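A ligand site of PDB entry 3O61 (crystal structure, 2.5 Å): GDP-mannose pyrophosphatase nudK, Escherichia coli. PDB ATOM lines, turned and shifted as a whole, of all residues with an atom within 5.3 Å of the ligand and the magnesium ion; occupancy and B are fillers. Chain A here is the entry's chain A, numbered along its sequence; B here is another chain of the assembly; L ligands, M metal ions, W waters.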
ATOM      1  N   TYR A  17      -1.085  19.261 -24.196  1.00  0.00           N
ATOM      2  CA  TYR A  17      -0.221  20.024 -23.325  1.00  0.00           C
ATOM      3  C   TYR A  17       1.226  19.610 -23.545  1.00  0.00           C
ATOM      4  O   TYR A  17       2.118  20.440 -23.745  1.00  0.00           O
ATOM      5  CB  TYR A  17      -0.642  19.805 -21.868  1.00  0.00           C
ATOM      6  CG  TYR A  17      -0.084  20.830 -20.905  1.00  0.00           C
ATOM      7  CD1 TYR A  17      -0.779  22.020 -20.636  1.00  0.00           C
ATOM      8  CD2 TYR A  17       1.134  20.635 -20.279  1.00  0.00           C
ATOM      9  CE1 TYR A  17      -0.262  22.986 -19.763  1.00  0.00           C
ATOM     10  CE2 TYR A  17       1.670  21.593 -19.397  1.00  0.00           C
ATOM     11  CZ  TYR A  17       0.958  22.762 -19.145  1.00  0.00           C
ATOM     12  OH  TYR A  17       1.482  23.687 -18.255  1.00  0.00           O
ATOM     13  N   PHE A  18       1.476  18.318 -23.463  1.00  0.00           N
ATOM     14  CA  PHE A  18       2.771  17.798 -23.860  1.00  0.00           C
ATOM     15  C   PHE A  18       2.473  16.878 -25.024  1.00  0.00           C
ATOM     16  O   PHE A  18       1.328  16.794 -25.449  1.00  0.00           O
ATOM     17  CB  PHE A  18       3.436  17.068 -22.682  1.00  0.00           C
ATOM     18  CG  PHE A  18       3.803  17.963 -21.519  1.00  0.00           C
ATOM     19  CD1 PHE A  18       4.754  18.976 -21.662  1.00  0.00           C
ATOM     20  CD2 PHE A  18       3.237  17.764 -20.277  1.00  0.00           C
ATOM     21  CE1 PHE A  18       5.111  19.811 -20.587  1.00  0.00           C
ATOM     22  CE2 PHE A  18       3.595  18.578 -19.189  1.00  0.00           C
ATOM     23  CZ  PHE A  18       4.544  19.597 -19.344  1.00  0.00           C
ATOM     24  N   ARG A  44       7.731  15.318 -22.370  1.00  0.00           N
ATOM     25  CA  ARG A  44       7.412  16.463 -21.525  1.00  0.00           C
ATOM     26  C   ARG A  44       8.574  17.436 -21.337  1.00  0.00           C
ATOM     27  O   ARG A  44       8.512  18.319 -20.485  1.00  0.00           O
ATOM     28  CB  ARG A  44       6.784  16.074 -20.155  1.00  0.00           C
ATOM     29  CG  ARG A  44       6.755  14.608 -19.831  1.00  0.00           C
ATOM     30  CD  ARG A  44       6.668  14.344 -18.328  1.00  0.00           C
ATOM     31  NE  ARG A  44       5.549  15.062 -17.717  1.00  0.00           N
ATOM     32  CZ  ARG A  44       5.681  15.927 -16.707  1.00  0.00           C
ATOM     33  NH1 ARG A  44       6.888  16.175 -16.180  1.00  0.00           N
ATOM     34  NH2 ARG A  44       4.605  16.545 -16.224  1.00  0.00           N
ATOM     35  N   GLY A  45       9.616  17.323 -22.150  1.00  0.00           N
ATOM     36  CA  GLY A  45      10.744  18.232 -22.015  1.00  0.00           C
ATOM     37  C   GLY A  45      11.660  17.733 -20.921  1.00  0.00           C
ATOM     38  O   GLY A  45      11.352  16.774 -20.205  1.00  0.00           O
ATOM     39  N   ASN A  46      12.824  18.334 -20.805  1.00  0.00           N
ATOM     40  CA  ASN A  46      13.759  17.931 -19.784  1.00  0.00           C
ATOM     41  C   ASN A  46      13.510  18.709 -18.483  1.00  0.00           C
ATOM     42  O   ASN A  46      12.633  19.580 -18.444  1.00  0.00           O
ATOM     43  CB  ASN A  46      15.184  18.042 -20.341  1.00  0.00           C
ATOM     44  CG  ASN A  46      15.386  17.142 -21.578  1.00  0.00           C
ATOM     45  OD1 ASN A  46      14.918  15.989 -21.624  1.00  0.00           O
ATOM     46  ND2 ASN A  46      16.037  17.679 -22.611  1.00  0.00           N
ATOM     47  N   GLY A  47      14.232  18.361 -17.426  1.00  0.00           N
ATOM     48  CA  GLY A  47      14.051  19.002 -16.098  1.00  0.00           C
ATOM     49  C   GLY A  47      15.380  19.139 -15.359  1.00  0.00           C
ATOM     50  O   GLY A  47      16.398  18.686 -15.856  1.00  0.00           O
ATOM     51  N   ALA A  48      15.377  19.791 -14.196  1.00  0.00           N
ATOM     52  CA  ALA A  48      16.534  19.816 -13.316  1.00  0.00           C
ATOM     53  C   ALA A  48      16.048  19.741 -11.874  1.00  0.00           C
ATOM     54  O   ALA A  48      14.956  20.240 -11.543  1.00  0.00           O
ATOM     55  CB  ALA A  48      17.320  21.061 -13.523  1.00  0.00           C
ATOM     56  N   THR A  49      16.859  19.102 -11.032  1.00  0.00           N
ATOM     57  CA  THR A  49      16.549  18.975  -9.610  1.00  0.00           C
ATOM     58  C   THR A  49      17.794  19.305  -8.768  1.00  0.00           C
ATOM     59  O   THR A  49      18.948  19.117  -9.203  1.00  0.00           O
ATOM     60  CB  THR A  49      15.980  17.589  -9.259  1.00  0.00           C
ATOM     61  OG1 THR A  49      15.708  17.507  -7.868  1.00  0.00           O
ATOM     62  CG2 THR A  49      16.941  16.444  -9.626  1.00  0.00           C
ATOM     63  N   ILE A  63      11.301  19.379  -0.533  1.00  0.00           N
ATOM     64  CA  ILE A  63       9.924  19.836  -0.548  1.00  0.00           C
ATOM     65  C   ILE A  63       8.903  18.682  -0.469  1.00  0.00           C
ATOM     66  O   ILE A  63       9.249  17.512  -0.387  1.00  0.00           O
ATOM     67  CB  ILE A  63       9.675  20.674  -1.807  1.00  0.00           C
ATOM     68  CG1 ILE A  63       9.886  19.801  -3.063  1.00  0.00           C
ATOM     69  CG2 ILE A  63      10.555  21.946  -1.780  1.00  0.00           C
ATOM     70  CD1 ILE A  63      10.082  20.572  -4.326  1.00  0.00           C
ATOM     71  N   GLN A  65       4.712  18.122  -2.140  1.00  0.00           N
ATOM     72  CA  GLN A  65       3.615  18.672  -2.913  1.00  0.00           C
ATOM     73  C   GLN A  65       2.742  17.523  -3.380  1.00  0.00           C
ATOM     74  O   GLN A  65       3.157  16.362  -3.314  1.00  0.00           O
ATOM     75  CB  GLN A  65       4.147  19.514  -4.092  1.00  0.00           C
ATOM     76  CG  GLN A  65       4.965  18.743  -5.175  1.00  0.00           C
ATOM     77  CD  GLN A  65       5.611  19.686  -6.181  1.00  0.00           C
ATOM     78  OE1 GLN A  65       5.027  20.709  -6.529  1.00  0.00           O
ATOM     79  NE2 GLN A  65       6.830  19.374  -6.613  1.00  0.00           N
ATOM     80  N   ARG A  67       1.296  15.069  -5.898  1.00  0.00           N
ATOM     81  CA  ARG A  67       1.572  14.523  -7.225  1.00  0.00           C
ATOM     82  C   ARG A  67       0.422  13.624  -7.652  1.00  0.00           C
ATOM     83  O   ARG A  67       0.356  12.469  -7.234  1.00  0.00           O
ATOM     84  CB  ARG A  67       2.882  13.728  -7.227  1.00  0.00           C
ATOM     85  CG  ARG A  67       4.132  14.530  -7.132  1.00  0.00           C
ATOM     86  CD  ARG A  67       4.186  15.660  -8.140  1.00  0.00           C
ATOM     87  NE  ARG A  67       5.518  16.254  -8.149  1.00  0.00           N
ATOM     88  CZ  ARG A  67       5.894  17.204  -8.988  1.00  0.00           C
ATOM     89  NH1 ARG A  67       5.026  17.652  -9.874  1.00  0.00           N
ATOM     90  NH2 ARG A  67       7.134  17.698  -8.952  1.00  0.00           N
ATOM     91  N   GLU A  82      10.328  15.152  -1.983  1.00  0.00           N
ATOM     92  CA  GLU A  82      11.164  15.205  -3.166  1.00  0.00           C
ATOM     93  C   GLU A  82      12.139  16.321  -3.013  1.00  0.00           C
ATOM     94  O   GLU A  82      11.890  17.308  -2.291  1.00  0.00           O
ATOM     95  CB  GLU A  82      10.349  15.615  -4.376  1.00  0.00           C
ATOM     96  CG  GLU A  82       9.698  14.561  -5.159  1.00  0.00           C
ATOM     97  CD  GLU A  82       8.549  15.136  -5.933  1.00  0.00           C
ATOM     98  OE1 GLU A  82       8.745  15.600  -7.078  1.00  0.00           O
ATOM     99  OE2 GLU A  82       7.443  15.149  -5.358  1.00  0.00           O
ATOM    100  N   ALA A  85      12.719  20.764  -7.759  1.00  0.00           N
ATOM    101  CA  ALA A  85      12.808  20.406  -9.210  1.00  0.00           C
ATOM    102  C   ALA A  85      11.912  21.267 -10.103  1.00  0.00           C
ATOM    103  O   ALA A  85      10.828  21.698  -9.687  1.00  0.00           O
ATOM    104  CB  ALA A  85      12.477  18.912  -9.426  1.00  0.00           C
ATOM    105  N   GLY A  86      12.349  21.503 -11.326  1.00  0.00           N
ATOM    106  CA  GLY A  86      11.600  22.341 -12.242  1.00  0.00           C
ATOM    107  C   GLY A  86      11.819  21.871 -13.663  1.00  0.00           C
ATOM    108  O   GLY A  86      12.795  21.169 -13.921  1.00  0.00           O
ATOM    109  N   LEU A  87      10.909  22.193 -14.570  1.00  0.00           N
ATOM    110  CA  LEU A  87      11.152  21.934 -15.994  1.00  0.00           C
ATOM    111  C   LEU A  87      12.054  23.023 -16.576  1.00  0.00           C
ATOM    112  O   LEU A  87      12.072  24.176 -16.123  1.00  0.00           O
ATOM    113  CB  LEU A  87       9.838  21.852 -16.763  1.00  0.00           C
ATOM    114  CG  LEU A  87       8.958  20.620 -16.532  1.00  0.00           C
ATOM    115  CD1 LEU A  87       7.526  20.959 -16.878  1.00  0.00           C
ATOM    116  CD2 LEU A  87       9.450  19.487 -17.369  1.00  0.00           C
ATOM    117  N   GLU A 104      10.480  27.629  -5.046  1.00  0.00           N
ATOM    118  CA  GLU A 104       9.974  26.483  -4.315  1.00  0.00           C
ATOM    119  C   GLU A 104      10.505  26.444  -2.891  1.00  0.00           C
ATOM    120  O   GLU A 104       9.734  26.242  -1.964  1.00  0.00           O
ATOM    121  CB  GLU A 104      10.278  25.158  -5.067  1.00  0.00           C
ATOM    122  CG  GLU A 104       9.855  25.210  -6.544  1.00  0.00           C
ATOM    123  CD  GLU A 104       9.674  23.851  -7.228  1.00  0.00           C
ATOM    124  OE1 GLU A 104       9.969  22.791  -6.619  1.00  0.00           O
ATOM    125  OE2 GLU A 104       9.229  23.846  -8.405  1.00  0.00           O
ATOM    126  N   GLU A 127      12.362  12.371 -21.108  1.00  0.00           N
ATOM    127  CA  GLU A 127      12.850  13.167 -19.964  1.00  0.00           C
ATOM    128  C   GLU A 127      14.318  12.956 -19.547  1.00  0.00           C
ATOM    129  O   GLU A 127      14.695  11.871 -19.098  1.00  0.00           O
ATOM    130  CB  GLU A 127      11.873  12.957 -18.808  1.00  0.00           C
ATOM    131  CG  GLU A 127      12.340  13.345 -17.450  1.00  0.00           C
ATOM    132  CD  GLU A 127      11.168  13.542 -16.469  1.00  0.00           C
ATOM    133  OE1 GLU A 127      10.579  14.659 -16.454  1.00  0.00           O
ATOM    134  OE2 GLU A 127      10.862  12.599 -15.720  1.00  0.00           O
ATOM    135  N   ILE A 129      17.163  14.517 -16.922  1.00  0.00           N
ATOM    136  CA  ILE A 129      17.179  15.250 -15.669  1.00  0.00           C
ATOM    137  C   ILE A 129      18.570  15.640 -15.237  1.00  0.00           C
ATOM    138  O   ILE A 129      19.407  14.760 -15.020  1.00  0.00           O
ATOM    139  CB  ILE A 129      16.512  14.470 -14.529  1.00  0.00           C
ATOM    140  CG1 ILE A 129      15.065  14.186 -14.894  1.00  0.00           C
ATOM    141  CG2 ILE A 129      16.543  15.290 -13.232  1.00  0.00           C
ATOM    142  CD1 ILE A 129      14.235  15.508 -15.017  1.00  0.00           C
ATOM    143  N   GLU A 151       1.263  27.633  -4.868  1.00  0.00           N
ATOM    144  CA  GLU A 151       1.146  26.182  -4.789  1.00  0.00           C
ATOM    145  C   GLU A 151       1.295  25.619  -3.362  1.00  0.00           C
ATOM    146  O   GLU A 151       1.933  26.224  -2.479  1.00  0.00           O
ATOM    147  CB  GLU A 151       2.155  25.485  -5.719  1.00  0.00           C
ATOM    148  CG  GLU A 151       1.850  25.586  -7.215  1.00  0.00           C
ATOM    149  CD  GLU A 151       2.807  26.516  -7.959  1.00  0.00           C
ATOM    150  OE1 GLU A 151       2.757  27.749  -7.702  1.00  0.00           O
ATOM    151  OE2 GLU A 151       3.594  26.026  -8.801  1.00  0.00           O
ATOM    152  N   ILE A 153       3.221  23.810  -2.112  1.00  0.00           N
ATOM    153  CA  ILE A 153       4.598  23.314  -1.867  1.00  0.00           C
ATOM    154  C   ILE A 153       5.086  23.674  -0.455  1.00  0.00           C
ATOM    155  O   ILE A 153       5.284  24.854  -0.133  1.00  0.00           O
ATOM    156  CB  ILE A 153       5.609  23.758  -2.959  1.00  0.00           C
ATOM    157  CG1 ILE A 153       5.216  23.217  -4.340  1.00  0.00           C
ATOM    158  CG2 ILE A 153       6.990  23.266  -2.614  1.00  0.00           C
ATOM    159  CD1 ILE A 153       5.979  23.842  -5.484  1.00  0.00           C
ATOM    160  N   ASP A 174      10.699   8.704  -4.121  1.00  0.00           N
ATOM    161  CA  ASP A 174      10.822   9.337  -5.405  1.00  0.00           C
ATOM    162  C   ASP A 174      12.215   8.993  -5.870  1.00  0.00           C
ATOM    163  O   ASP A 174      13.097   8.874  -5.043  1.00  0.00           O
ATOM    164  CB  ASP A 174      10.691  10.867  -5.257  1.00  0.00           C
ATOM    165  CG  ASP A 174      10.978  11.581  -6.575  1.00  0.00           C
ATOM    166  OD1 ASP A 174      10.492  11.082  -7.607  1.00  0.00           O
ATOM    167  OD2 ASP A 174      11.726  12.590  -6.586  1.00  0.00           O
ATOM    168  N   LYS A 176      14.602  10.563  -8.238  1.00  0.00           N
ATOM    169  CA  LYS A 176      15.591  11.627  -8.270  1.00  0.00           C
ATOM    170  C   LYS A 176      15.951  12.087  -6.853  1.00  0.00           C
ATOM    171  O   LYS A 176      17.080  12.497  -6.599  1.00  0.00           O
ATOM    172  CB  LYS A 176      15.082  12.800  -9.161  1.00  0.00           C
ATOM    173  CG  LYS A 176      13.747  13.388  -8.720  1.00  0.00           C
ATOM    174  CD  LYS A 176      13.558  14.847  -9.147  1.00  0.00           C
ATOM    175  CE  LYS A 176      12.379  15.482  -8.382  1.00  0.00           C
ATOM    176  NZ  LYS A 176      11.131  14.651  -8.355  1.00  0.00           N
ATOM    177  N   LYS B  38      -5.839  20.806 -13.690  1.00  0.00           N
ATOM    178  CA  LYS B  38      -5.829  19.836 -14.807  1.00  0.00           C
ATOM    179  C   LYS B  38      -4.369  19.358 -15.007  1.00  0.00           C
ATOM    180  O   LYS B  38      -3.467  20.181 -15.016  1.00  0.00           O
ATOM    181  CB  LYS B  38      -6.402  20.464 -16.081  1.00  0.00           C
ATOM    182  CG  LYS B  38      -7.909  20.178 -16.396  1.00  0.00           C
ATOM    183  CD  LYS B  38      -8.308  20.685 -17.816  1.00  0.00           C
ATOM    184  CE  LYS B  38      -9.765  20.327 -18.235  1.00  0.00           C
ATOM    185  NZ  LYS B  38      -9.849  19.149 -19.205  1.00  0.00           N
ATOM    186  N   ARG B  39      -4.147  18.043 -15.153  1.00  0.00           N
ATOM    187  CA  ARG B  39      -2.775  17.483 -15.242  1.00  0.00           C
ATOM    188  C   ARG B  39      -2.722  16.312 -16.209  1.00  0.00           C
ATOM    189  O   ARG B  39      -3.534  15.396 -16.111  1.00  0.00           O
ATOM    190  CB  ARG B  39      -2.261  16.974 -13.893  1.00  0.00           C
ATOM    191  CG  ARG B  39      -1.742  17.997 -12.859  1.00  0.00           C
ATOM    192  CD  ARG B  39      -0.507  18.810 -13.325  1.00  0.00           C
ATOM    193  NE  ARG B  39      -0.013  19.652 -12.247  1.00  0.00           N
ATOM    194  CZ  ARG B  39      -0.581  20.799 -11.845  1.00  0.00           C
ATOM    195  NH1 ARG B  39      -1.684  21.259 -12.429  1.00  0.00           N
ATOM    196  NH2 ARG B  39      -0.047  21.479 -10.837  1.00  0.00           N
ATOM    197  N   GLU B  40      -1.759  16.298 -17.117  1.00  0.00           N
ATOM    198  CA  GLU B  40      -1.623  15.155 -17.985  1.00  0.00           C
ATOM    199  C   GLU B  40      -0.945  14.060 -17.212  1.00  0.00           C
ATOM    200  O   GLU B  40       0.100  14.326 -16.646  1.00  0.00           O
ATOM    201  CB  GLU B  40      -0.803  15.476 -19.215  1.00  0.00           C
ATOM    202  CG  GLU B  40      -1.568  16.209 -20.283  1.00  0.00           C
ATOM    203  CD  GLU B  40      -0.936  16.046 -21.636  1.00  0.00           C
ATOM    204  OE1 GLU B  40       0.235  15.582 -21.719  1.00  0.00           O
ATOM    205  OE2 GLU B  40      -1.602  16.401 -22.627  1.00  0.00           O
ATOM    206  N   MET B 120       9.534   7.113 -10.623  1.00  0.00           N
ATOM    207  CA  MET B 120      10.676   7.585 -11.389  1.00  0.00           C
ATOM    208  C   MET B 120      10.468   8.967 -11.993  1.00  0.00           C
ATOM    209  O   MET B 120      11.400   9.756 -12.075  1.00  0.00           O
ATOM    210  CB  MET B 120      11.085   6.595 -12.468  1.00  0.00           C
ATOM    211  CG  MET B 120      11.821   5.322 -11.974  1.00  0.00           C
ATOM    212  SD  MET B 120      13.453   5.599 -11.215  1.00  0.00           S
ATOM    213  CE  MET B 120      12.874   5.936  -9.556  1.00  0.00           C
ATOM    214  N   SER B 121       9.252   9.285 -12.398  1.00  0.00           N
ATOM    215  CA  SER B 121       9.000  10.592 -12.960  1.00  0.00           C
ATOM    216  C   SER B 121       7.591  11.062 -12.554  1.00  0.00           C
ATOM    217  O   SER B 121       6.635  10.974 -13.333  1.00  0.00           O
ATOM    218  CB  SER B 121       9.174  10.497 -14.479  1.00  0.00           C
ATOM    219  OG  SER B 121       8.845  11.714 -15.102  1.00  0.00           O
ATOM    220  N   PRO B 122       7.430  11.486 -11.290  1.00  0.00           N
ATOM    221  CA  PRO B 122       6.086  11.767 -10.746  1.00  0.00           C
ATOM    222  C   PRO B 122       5.430  13.057 -11.228  1.00  0.00           C
ATOM    223  O   PRO B 122       4.425  13.504 -10.672  1.00  0.00           O
ATOM    224  CB  PRO B 122       6.335  11.783  -9.217  1.00  0.00           C
ATOM    225  CG  PRO B 122       7.738  12.105  -9.036  1.00  0.00           C
ATOM    226  CD  PRO B 122       8.489  11.664 -10.277  1.00  0.00           C
ATOM    227  N   GLY B 123       5.978  13.671 -12.266  1.00  0.00           N
ATOM    228  CA  GLY B 123       5.337  14.842 -12.865  1.00  0.00           C
ATOM    229  C   GLY B 123       4.089  14.349 -13.534  1.00  0.00           C
ATOM    230  O   GLY B 123       2.978  14.682 -13.135  1.00  0.00           O
HETATM  231  N1  LIG L   1      -2.466  22.091 -17.134  1.00  0.00           N
HETATM  232  C1  LIG L   1      -1.291  21.445 -16.844  1.00  0.00           C
HETATM  233  N2  LIG L   1      -1.135  20.126 -17.159  1.00  0.00           N
HETATM  234  N3  LIG L   1      -0.307  22.148 -16.224  1.00  0.00           N
HETATM  235  C2  LIG L   1       0.898  21.601 -15.884  1.00  0.00           C
HETATM  236  C3  LIG L   1       1.122  20.172 -16.207  1.00  0.00           C
HETATM  237  C4  LIG L   1       0.006  19.431 -16.881  1.00  0.00           C
HETATM  238  O1  LIG L   1       0.121  18.227 -17.199  1.00  0.00           O
HETATM  239  N4  LIG L   1       2.375  19.896 -15.778  1.00  0.00           N
HETATM  240  C5  LIG L   1       2.891  21.025 -15.232  1.00  0.00           C
HETATM  241  N5  LIG L   1       2.021  22.055 -15.287  1.00  0.00           N
HETATM  242  C6  LIG L   1       2.291  23.445 -14.774  1.00  0.00           C
HETATM  243  C7  LIG L   1       1.539  23.747 -13.470  1.00  0.00           C
HETATM  244  O2  LIG L   1       1.254  25.156 -13.368  1.00  0.00           O
HETATM  245  C8  LIG L   1       2.527  23.329 -12.393  1.00  0.00           C
HETATM  246  O3  LIG L   1       2.316  24.025 -11.136  1.00  0.00           O
HETATM  247  C9  LIG L   1       3.885  23.596 -13.033  1.00  0.00           C
HETATM  248  O4  LIG L   1       3.680  23.588 -14.468  1.00  0.00           O
HETATM  249  C10 LIG L   1       4.986  22.604 -12.632  1.00  0.00           C
HETATM  250  O5  LIG L   1       6.268  23.269 -12.699  1.00  0.00           O
HETATM  251  P1  LIG L   1       7.681  22.594 -12.263  1.00  0.00           P
HETATM  252  O6  LIG L   1       7.992  22.881 -10.802  1.00  0.00           O
HETATM  253  O7  LIG L   1       8.672  22.983 -13.349  1.00  0.00           O
HETATM  254  O8  LIG L   1       7.274  21.007 -12.451  1.00  0.00           O
HETATM  255  P2  LIG L   1       7.667  19.728 -11.515  1.00  0.00           P
HETATM  256  O9  LIG L   1       8.309  20.071 -10.156  1.00  0.00           O
HETATM  257  O10 LIG L   1       6.414  18.852 -11.552  1.00  0.00           O
HETATM  258  O11 LIG L   1       8.779  19.053 -12.468  1.00  0.00           O
HETATM  259  C11 LIG L   1      10.084  18.579 -12.124  1.00  0.00           C
HETATM  260  O12 LIG L   1      10.059  17.313 -11.431  1.00  0.00           O
HETATM  261  C12 LIG L   1       9.547  16.196 -12.184  1.00  0.00           C
HETATM  262  C13 LIG L   1       9.458  14.919 -11.322  1.00  0.00           C
HETATM  263  O13 LIG L   1      10.629  14.085 -11.435  1.00  0.00           O
HETATM  264  C14 LIG L   1      10.831  18.467 -13.454  1.00  0.00           C
HETATM  265  O14 LIG L   1      12.219  18.325 -13.206  1.00  0.00           O
HETATM  266  C15 LIG L   1      10.334  17.267 -14.304  1.00  0.00           C
HETATM  267  O15 LIG L   1      11.174  17.172 -15.454  1.00  0.00           O
HETATM  268  C16 LIG L   1      10.363  15.983 -13.467  1.00  0.00           C
HETATM  269  O16 LIG L   1       9.857  14.819 -14.148  1.00  0.00           O
HETATM  270 MG    MG M   1       8.686  21.634  -8.925  1.00  0.00          MG
HETATM  271  O   HOH W   1       9.344  20.199  -7.682  1.00  0.00           O
HETATM  272  O   HOH W   2       3.236  21.549  -9.855  1.00  0.00           O
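The backbone carbonyl oxygen (O) of Gly 86 sits at hydrogen-bond distance from an oxygen (O14) of the ligand (3.0 Å).
N of Glu 40 of chain B is in hydrogen-bond range of O1 of the ligand.
The side-chain carboxylate of Glu 151 is in hydrogen-bond range of an oxygen (O3) of the ligand.
N of Leu 87 lies within hydrogen-bond range of O7 of the ligand (2.7 Å).
The side-chain amino group (NZ) of Lys 176 sits at hydrogen-bond distance from an oxygen (O13) of the ligand (3.2 Å).
OG of Ser 121 of chain B is in hydrogen-bond range of O16 of the ligand (3.4 Å).
N3 of the ligand is in hydrogen-bond range of OH of Tyr 17.
The side-chain carboxylate (OE1) of Glu 127 lies within hydrogen-bond range of an oxygen (O16) of the ligand (2.4 Å).
O3 of the ligand lies within hydrogen-bond range of NH2 of Arg 39 of chain B, at 3.5 Å.
The backbone carbonyl oxygen of Lys 38 of chain B sits at hydrogen-bond distance from a nitrogen (N1) of the ligand (3.0 Å).
The guanidinium group (NH1) of Arg 67 is in salt-bridge range of an oxygen (O10) of the ligand.
Water W1 lies within hydrogen-bond range of NE2 of Gln 65 (2.9 Å), OE1 of Glu 104 (2.9 Å) and N of Ala 85 (3.4 Å).
Water W2 bridges O3 of the ligand (2.9 Å) and NH2 of Arg 39 of chain B (3.4 Å).
The backbone NH (N) of Gly 86 sits at hydrogen-bond distance from the backbone carbonyl oxygen (O) of Ala 48, at 2.9 Å.
N of Tyr 17 lies within hydrogen-bond range of OE2 of Glu 40 of chain B, 3.3 Å away.
The side-chain amide nitrogen (NE2) of Gln 65 sits close to the guanidinium group (NH2) of Arg 67 (2.9 Å).
The side-chain amino group (NZ) of Lys 176 lies within salt-bridge range of the side-chain carboxylate (OD2) of Asp 174 (2.8 Å).
The guanidinium group (NH2) of Arg 67 lies within salt-bridge range of the side-chain carboxylate (OE1) of Glu 82 (3.2 Å).
The side-chain amino group of Lys 176 lies within salt-bridge range of the side-chain carboxylate of Glu 82 (2.9 Å).
The side-chain carboxylate (OE1) of Glu 40 of chain B is in hydrogen-bond range of the backbone NH (N) of Phe 18, 3.5 Å away.
The magnesium ion is bound by water W1 (2.0 Å), O9 of the ligand (2.0 Å), O of Ala 85 (2.3 Å), OE2 of Glu 104 (2.3 Å) and O6 of the ligand (2.4 Å).
The magnesium ion has five donor atoms within binding distance.
Residues that only touch the magnesium ion: Gln 65 (3.7 Å).
Of the 29 residues printed, 3 come within 4 Å of the magnesium ion.
Along chain A the residues within 4 Å of the magnesium ion span positions 65 to 104.
The nearest printed residue that does not touch the magnesium ion is Arg 67 (4.2 Å).
Merely in contact with the ligand: Pro 122 of chain B, Gly 47, Ile 129, Ala 48, Gly 123 of chain B, Arg 44, Phe 18 and Gln 65.
Hydrophobic or aromatic side chains that line the ligand: Tyr 17, Phe 18, Ala 85, Leu 87, Ile 129 and Pro 122 of chain B.
21 residues have an atom within 4 Å of the ligand: Tyr 17, Phe 18, Arg 44, Gly 47, Ala 48, Gln 65, Arg 67, Ala 85, Gly 86, Leu 87, Glu 104, Glu 127, Ile 129, Glu 151, Lys 176, Lys 38 of chain B, Arg 39 of chain B, Glu 40 of chain B, Ser 121 of chain B, Pro 122 of chain B and Gly 123 of chain B.
The nearest printed residue that does not touch the ligand is Asn 46 (4.1 Å).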
